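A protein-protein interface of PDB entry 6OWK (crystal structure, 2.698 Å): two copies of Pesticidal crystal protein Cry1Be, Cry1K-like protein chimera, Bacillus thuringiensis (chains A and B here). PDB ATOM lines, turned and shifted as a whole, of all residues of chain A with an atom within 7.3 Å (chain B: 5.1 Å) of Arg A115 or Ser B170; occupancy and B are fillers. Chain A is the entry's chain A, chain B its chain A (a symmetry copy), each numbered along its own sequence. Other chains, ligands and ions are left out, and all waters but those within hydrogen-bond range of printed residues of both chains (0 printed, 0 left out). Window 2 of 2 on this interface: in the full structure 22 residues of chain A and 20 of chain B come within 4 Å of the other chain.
Position printed for both chains: 121. Of the 9 pairs that touch across the chains among the printed residues, none has its exchanged pair printed and touching as well.
The side-chain hydroxyl of Tyr B121 lies within hydrogen-bond range of the backbone carbonyl oxygen of Gly B173, at 3.0 Å. The backbone carbonyl oxygen (O) of Gly B169 lies close to the backbone NH (N) of Leu B174 (3.2 Å). The backbone NH of Thr A116 is in hydrogen-bond range of the side-chain carboxylate of Asp A113 (3.0 Å). The side-chain carboxylate of Asp A113 sits at hydrogen-bond distance from the backbone NH of Arg A115. OD1 of Asn A110 is in hydrogen-bond range of OG1 of Thr A116 (3.1 Å).
Among the printed residues, pairs that only touch across the chains: Val A119 with Tyr B121, Thr A116 with Thr B175, Arg A115 with Ser B170, Asp A113 with Thr B175 and Arg A115 with Thr B175.
Of the 12 printed residues of chain B, 5 touch a printed residue of chain A. Printed residues of chain B that touch a printed residue of chain A: Tyr B121, Ser B170, Gly B173, Leu B174 and Thr B175. Hydrophobic or aromatic side chains of chain B that line the printed part of chain A: Tyr B121. Of the 11 printed residues of chain A, 5 touch a printed residue of chain B. Among the printed residues, no Asp or Glu carboxylate lies within 4 Å of a Lys or Arg side-chain nitrogen of the other chain.
The backbone carbonyl oxygen (O) of Gly B173 lies close to the guanidinium group (NE) of Arg A115. O of Leu B174 lies within hydrogen-bond range of NH1 of Arg A115, 2.7 Å away. OH of Tyr B121 sits at hydrogen-bond distance from OG of Ser A118 (3.2 Å). The backbone carbonyl oxygen of Arg A115 lies within hydrogen-bond range of the side-chain hydroxyl of Tyr B121 (3.3 Å).
Arg A115 touches just these residues of chain B: Tyr B121 (3.3 Å), Ser B170 (3.7 Å), Gly B173 (3.1 Å), Leu B174 (2.7 Å) and Thr B175 (3.9 Å). Of the printed residues of chain A, Leu B174 touches Arg A115. Of the printed residues of chain B, Asp A113 touches Thr B175. Of the printed residues of chain B, Thr A116 touches Thr B175. Of the printed residues of chain A, Thr B175 touches Asp A113 (3.9 Å), Arg A115 (3.9 Å) and Thr A116 (3.5 Å). Of the printed residues of chain B, Val A119 touches Tyr B121. Phe B168 touches none of the printed residues of chain A. The nearest printed residue of chain A that does not touch Ser B170 is Val A119 (9.8 Å). The nearest printed residue of chain B that does not touch Thr A116 is Tyr B121 (5.3 Å).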
ATOM      1  N   ASN A 110      -7.081  10.259   4.757  1.00  0.00           N
ATOM      2  CA  ASN A 110      -6.442   9.441   5.778  1.00  0.00           C
ATOM      3  C   ASN A 110      -7.001   8.025   5.773  1.00  0.00           C
ATOM      4  O   ASN A 110      -8.214   7.819   5.689  1.00  0.00           O
ATOM      5  CB  ASN A 110      -6.632  10.064   7.162  1.00  0.00           C
ATOM      6  CG  ASN A 110      -5.532  11.046   7.518  1.00  0.00           C
ATOM      7  OD1 ASN A 110      -4.913  10.944   8.580  1.00  0.00           O
ATOM      8  ND2 ASN A 110      -5.283  12.003   6.635  1.00  0.00           N
ATOM      9  N   ASP A 112      -4.841   5.427   7.876  1.00  0.00           N
ATOM     10  CA  ASP A 112      -4.347   4.992   9.175  1.00  0.00           C
ATOM     11  C   ASP A 112      -3.694   6.170   9.882  1.00  0.00           C
ATOM     12  O   ASP A 112      -2.818   6.829   9.314  1.00  0.00           O
ATOM     13  CB  ASP A 112      -3.343   3.842   9.044  1.00  0.00           C
ATOM     14  CG  ASP A 112      -3.692   2.886   7.921  1.00  0.00           C
ATOM     15  OD1 ASP A 112      -2.914   2.807   6.946  1.00  0.00           O
ATOM     16  OD2 ASP A 112      -4.737   2.208   8.015  1.00  0.00           O
ATOM     17  N   ASP A 113      -4.124   6.422  11.117  1.00  0.00           N
ATOM     18  CA  ASP A 113      -3.522   7.435  11.974  1.00  0.00           C
ATOM     19  C   ASP A 113      -4.134   7.345  13.364  1.00  0.00           C
ATOM     20  O   ASP A 113      -5.357   7.430  13.519  1.00  0.00           O
ATOM     21  CB  ASP A 113      -3.713   8.841  11.396  1.00  0.00           C
ATOM     22  CG  ASP A 113      -2.735   9.850  11.976  1.00  0.00           C
ATOM     23  OD1 ASP A 113      -2.674   9.975  13.214  1.00  0.00           O
ATOM     24  OD2 ASP A 113      -2.035  10.527  11.193  1.00  0.00           O
ATOM     25  N   ALA A 114      -3.294   7.159  14.377  1.00  0.00           N
ATOM     26  CA  ALA A 114      -3.762   7.128  15.755  1.00  0.00           C
ATOM     27  C   ALA A 114      -3.962   8.520  16.341  1.00  0.00           C
ATOM     28  O   ALA A 114      -4.397   8.630  17.492  1.00  0.00           O
ATOM     29  CB  ALA A 114      -2.784   6.335  16.627  1.00  0.00           C
ATOM     30  N   ARG A 115      -3.660   9.576  15.586  1.00  0.00           N
ATOM     31  CA  ARG A 115      -3.823  10.954  16.038  1.00  0.00           C
ATOM     32  C   ARG A 115      -4.956  11.694  15.341  1.00  0.00           C
ATOM     33  O   ARG A 115      -5.718  12.401  16.006  1.00  0.00           O
ATOM     34  CB  ARG A 115      -2.518  11.737  15.840  1.00  0.00           C
ATOM     35  CG  ARG A 115      -1.341  11.243  16.677  1.00  0.00           C
ATOM     36  CD  ARG A 115      -0.066  12.007  16.328  1.00  0.00           C
ATOM     37  NE  ARG A 115       0.842  12.126  17.467  1.00  0.00           N
ATOM     38  CZ  ARG A 115       1.986  12.803  17.444  1.00  0.00           C
ATOM     39  NH1 ARG A 115       2.370  13.425  16.337  1.00  0.00           N
ATOM     40  NH2 ARG A 115       2.748  12.860  18.527  1.00  0.00           N
ATOM     41  N   THR A 116      -5.086  11.564  14.014  1.00  0.00           N
ATOM     42  CA  THR A 116      -6.188  12.222  13.310  1.00  0.00           C
ATOM     43  C   THR A 116      -7.528  11.643  13.741  1.00  0.00           C
ATOM     44  O   THR A 116      -8.434  12.380  14.145  1.00  0.00           O
ATOM     45  CB  THR A 116      -6.027  12.088  11.794  1.00  0.00           C
ATOM     46  OG1 THR A 116      -6.185  10.716  11.411  1.00  0.00           O
ATOM     47  CG2 THR A 116      -4.666  12.584  11.344  1.00  0.00           C
ATOM     48  N   ARG A 117      -7.669  10.320  13.662  1.00  0.00           N
ATOM     49  CA  ARG A 117      -8.838   9.658  14.226  1.00  0.00           C
ATOM     50  C   ARG A 117      -8.930   9.794  15.738  1.00  0.00           C
ATOM     51  O   ARG A 117      -9.859   9.228  16.315  1.00  0.00           O
ATOM     52  CB  ARG A 117      -8.838   8.177  13.851  1.00  0.00           C
ATOM     53  CG  ARG A 117      -8.382   7.891  12.432  1.00  0.00           C
ATOM     54  CD  ARG A 117      -8.689   6.461  12.046  1.00  0.00           C
ATOM     55  NE  ARG A 117      -9.005   6.345  10.628  1.00  0.00           N
ATOM     56  CZ  ARG A 117      -9.078   5.193   9.972  1.00  0.00           C
ATOM     57  NH1 ARG A 117      -8.861   4.051  10.609  1.00  0.00           N
ATOM     58  NH2 ARG A 117      -9.367   5.180   8.678  1.00  0.00           N
ATOM     59  N   SER A 118      -7.996  10.504  16.378  1.00  0.00           N
ATOM     60  CA  SER A 118      -8.034  10.797  17.805  1.00  0.00           C
ATOM     61  C   SER A 118      -8.392  12.242  18.113  1.00  0.00           C
ATOM     62  O   SER A 118      -8.979  12.505  19.164  1.00  0.00           O
ATOM     63  CB  SER A 118      -6.684  10.475  18.461  1.00  0.00           C
ATOM     64  OG  SER A 118      -6.733  10.605  19.872  1.00  0.00           O
ATOM     65  N   VAL A 119      -8.040  13.184  17.238  1.00  0.00           N
ATOM     66  CA  VAL A 119      -8.568  14.538  17.362  1.00  0.00           C
ATOM     67  C   VAL A 119      -9.970  14.614  16.775  1.00  0.00           C
ATOM     68  O   VAL A 119     -10.906  15.088  17.431  1.00  0.00           O
ATOM     69  CB  VAL A 119      -7.627  15.556  16.692  1.00  0.00           C
ATOM     70  CG1 VAL A 119      -8.209  16.953  16.819  1.00  0.00           C
ATOM     71  CG2 VAL A 119      -6.237  15.493  17.306  1.00  0.00           C
ATOM     72  N   LEU A 120     -10.129  14.147  15.531  1.00  0.00           N
ATOM     73  CA  LEU A 120     -11.449  14.078  14.909  1.00  0.00           C
ATOM     74  C   LEU A 120     -12.431  13.323  15.796  1.00  0.00           C
ATOM     75  O   LEU A 120     -13.584  13.740  15.953  1.00  0.00           O
ATOM     76  CB  LEU A 120     -11.330  13.428  13.529  1.00  0.00           C
ATOM     77  CG  LEU A 120     -12.559  12.837  12.842  1.00  0.00           C
ATOM     78  CD1 LEU A 120     -13.626  13.894  12.621  1.00  0.00           C
ATOM     79  CD2 LEU A 120     -12.142  12.214  11.525  1.00  0.00           C
ATOM     80  N   TYR A 121     -11.988  12.201  16.365  1.00  0.00           N
ATOM     81  CA  TYR A 121     -12.571  11.584  17.554  1.00  0.00           C
ATOM     82  C   TYR A 121     -13.168  12.625  18.489  1.00  0.00           C
ATOM     83  O   TYR A 121     -14.390  12.721  18.641  1.00  0.00           O
ATOM     84  CB  TYR A 121     -11.480  10.819  18.303  1.00  0.00           C
ATOM     85  CG  TYR A 121     -11.861   9.543  19.020  1.00  0.00           C
ATOM     86  CD1 TYR A 121     -12.994   9.465  19.812  1.00  0.00           C
ATOM     87  CD2 TYR A 121     -11.041   8.426  18.940  1.00  0.00           C
ATOM     88  CE1 TYR A 121     -13.315   8.290  20.481  1.00  0.00           C
ATOM     89  CE2 TYR A 121     -11.349   7.258  19.597  1.00  0.00           C
ATOM     90  CZ  TYR A 121     -12.486   7.191  20.367  1.00  0.00           C
ATOM     91  OH  TYR A 121     -12.787   6.020  21.022  1.00  0.00           O
ATOM     92  N   TYR B 121      -4.417  16.206  26.199  1.00  0.00           N
ATOM     93  CA  TYR B 121      -5.109  16.089  24.920  1.00  0.00           C
ATOM     94  C   TYR B 121      -6.520  16.652  24.993  1.00  0.00           C
ATOM     95  O   TYR B 121      -6.822  17.698  24.408  1.00  0.00           O
ATOM     96  CB  TYR B 121      -5.189  14.612  24.531  1.00  0.00           C
ATOM     97  CG  TYR B 121      -5.105  14.250  23.065  1.00  0.00           C
ATOM     98  CD1 TYR B 121      -5.827  14.937  22.104  1.00  0.00           C
ATOM     99  CD2 TYR B 121      -4.333  13.171  22.656  1.00  0.00           C
ATOM    100  CE1 TYR B 121      -5.754  14.574  20.765  1.00  0.00           C
ATOM    101  CE2 TYR B 121      -4.252  12.804  21.333  1.00  0.00           C
ATOM    102  CZ  TYR B 121      -4.963  13.506  20.389  1.00  0.00           C
ATOM    103  OH  TYR B 121      -4.879  13.132  19.068  1.00  0.00           O
ATOM    104  N   ALA B 165      -0.632  25.023  20.409  1.00  0.00           N
ATOM    105  CA  ALA B 165      -0.806  23.939  19.446  1.00  0.00           C
ATOM    106  C   ALA B 165       0.401  23.836  18.528  1.00  0.00           C
ATOM    107  O   ALA B 165       0.985  22.759  18.363  1.00  0.00           O
ATOM    108  CB  ALA B 165      -2.076  24.157  18.625  1.00  0.00           C
ATOM    109  N   SER B 166       0.788  24.958  17.918  1.00  0.00           N
ATOM    110  CA  SER B 166       1.966  24.976  17.059  1.00  0.00           C
ATOM    111  C   SER B 166       3.231  24.695  17.860  1.00  0.00           C
ATOM    112  O   SER B 166       4.094  23.920  17.430  1.00  0.00           O
ATOM    113  CB  SER B 166       2.074  26.329  16.352  1.00  0.00           C
ATOM    114  OG  SER B 166       0.794  26.847  16.027  1.00  0.00           O
ATOM    115  N   PHE B 168       4.109  23.049  20.842  1.00  0.00           N
ATOM    116  CA  PHE B 168       4.444  21.694  21.272  1.00  0.00           C
ATOM    117  C   PHE B 168       3.260  20.732  21.222  1.00  0.00           C
ATOM    118  O   PHE B 168       3.389  19.591  21.696  1.00  0.00           O
ATOM    119  CB  PHE B 168       5.030  21.710  22.686  1.00  0.00           C
ATOM    120  CG  PHE B 168       4.301  22.615  23.630  1.00  0.00           C
ATOM    121  CD1 PHE B 168       3.004  22.333  24.017  1.00  0.00           C
ATOM    122  CD2 PHE B 168       4.912  23.753  24.127  1.00  0.00           C
ATOM    123  CE1 PHE B 168       2.327  23.167  24.879  1.00  0.00           C
ATOM    124  CE2 PHE B 168       4.241  24.591  24.992  1.00  0.00           C
ATOM    125  CZ  PHE B 168       2.946  24.297  25.368  1.00  0.00           C
ATOM    126  N   GLY B 169       2.106  21.159  20.703  1.00  0.00           N
ATOM    127  CA  GLY B 169       1.098  20.202  20.270  1.00  0.00           C
ATOM    128  C   GLY B 169       1.644  19.113  19.366  1.00  0.00           C
ATOM    129  O   GLY B 169       1.142  17.986  19.403  1.00  0.00           O
ATOM    130  N   SER B 170       2.700  19.416  18.597  1.00  0.00           N
ATOM    131  CA  SER B 170       3.423  18.419  17.810  1.00  0.00           C
ATOM    132  C   SER B 170       3.936  17.272  18.666  1.00  0.00           C
ATOM    133  O   SER B 170       4.244  16.203  18.128  1.00  0.00           O
ATOM    134  CB  SER B 170       4.594  19.092  17.071  1.00  0.00           C
ATOM    135  OG  SER B 170       5.533  18.163  16.564  1.00  0.00           O
ATOM    136  N   GLU B 171       4.066  17.476  19.976  1.00  0.00           N
ATOM    137  CA  GLU B 171       4.419  16.405  20.901  1.00  0.00           C
ATOM    138  C   GLU B 171       3.223  15.875  21.680  1.00  0.00           C
ATOM    139  O   GLU B 171       3.230  14.709  22.086  1.00  0.00           O
ATOM    140  CB  GLU B 171       5.492  16.882  21.887  1.00  0.00           C
ATOM    141  CG  GLU B 171       6.212  15.757  22.601  1.00  0.00           C
ATOM    142  CD  GLU B 171       6.485  14.568  21.693  1.00  0.00           C
ATOM    143  OE1 GLU B 171       5.840  13.513  21.873  1.00  0.00           O
ATOM    144  OE2 GLU B 171       7.348  14.688  20.798  1.00  0.00           O
ATOM    145  N   PHE B 172       2.202  16.710  21.884  1.00  0.00           N
ATOM    146  CA  PHE B 172       0.945  16.346  22.537  1.00  0.00           C
ATOM    147  C   PHE B 172       0.415  14.982  22.121  1.00  0.00           C
ATOM    148  O   PHE B 172      -0.223  14.283  22.913  1.00  0.00           O
ATOM    149  CB  PHE B 172      -0.134  17.377  22.204  1.00  0.00           C
ATOM    150  CG  PHE B 172      -0.290  18.456  23.221  1.00  0.00           C
ATOM    151  CD1 PHE B 172       0.795  18.923  23.937  1.00  0.00           C
ATOM    152  CD2 PHE B 172      -1.534  19.019  23.449  1.00  0.00           C
ATOM    153  CE1 PHE B 172       0.640  19.928  24.871  1.00  0.00           C
ATOM    154  CE2 PHE B 172      -1.694  20.017  24.380  1.00  0.00           C
ATOM    155  CZ  PHE B 172      -0.609  20.476  25.089  1.00  0.00           C
ATOM    156  N   GLY B 173       0.668  14.611  20.880  1.00  0.00           N
ATOM    157  CA  GLY B 173      -0.115  13.624  20.186  1.00  0.00           C
ATOM    158  C   GLY B 173      -0.939  14.210  19.060  1.00  0.00           C
ATOM    159  O   GLY B 173      -1.941  13.599  18.670  1.00  0.00           O
ATOM    160  N   LEU B 174      -0.569  15.382  18.554  1.00  0.00           N
ATOM    161  CA  LEU B 174      -1.240  16.022  17.435  1.00  0.00           C
ATOM    162  C   LEU B 174      -0.521  15.679  16.138  1.00  0.00           C
ATOM    163  O   LEU B 174       0.705  15.545  16.100  1.00  0.00           O
ATOM    164  CB  LEU B 174      -1.281  17.543  17.607  1.00  0.00           C
ATOM    165  CG  LEU B 174      -2.510  18.188  18.248  1.00  0.00           C
ATOM    166  CD1 LEU B 174      -2.665  17.746  19.692  1.00  0.00           C
ATOM    167  CD2 LEU B 174      -2.414  19.704  18.160  1.00  0.00           C
ATOM    168  N   THR B 175      -1.299  15.541  15.073  1.00  0.00           N
ATOM    169  CA  THR B 175      -0.751  15.298  13.752  1.00  0.00           C
ATOM    170  C   THR B 175      -0.395  16.620  13.081  1.00  0.00           C
ATOM    171  O   THR B 175      -0.884  17.687  13.458  1.00  0.00           O
ATOM    172  CB  THR B 175      -1.749  14.528  12.890  1.00  0.00           C
ATOM    173  OG1 THR B 175      -1.202  14.327  11.582  1.00  0.00           O
ATOM    174  CG2 THR B 175      -3.040  15.308  12.776  1.00  0.00           C
ATOM    175  N   ILE B 179      -2.275  20.311  13.557  1.00  0.00           N
ATOM    176  CA  ILE B 179      -1.520  21.507  13.927  1.00  0.00           C
ATOM    177  C   ILE B 179      -1.799  22.624  12.933  1.00  0.00           C
ATOM    178  O   ILE B 179      -2.051  23.775  13.313  1.00  0.00           O
ATOM    179  CB  ILE B 179      -0.015  21.196  14.002  1.00  0.00           C
ATOM    180  CG1 ILE B 179       0.282  20.170  15.093  1.00  0.00           C
ATOM    181  CG2 ILE B 179       0.780  22.473  14.243  1.00  0.00           C
ATOM    182  CD1 ILE B 179       1.634  19.525  14.934  1.00  0.00           C
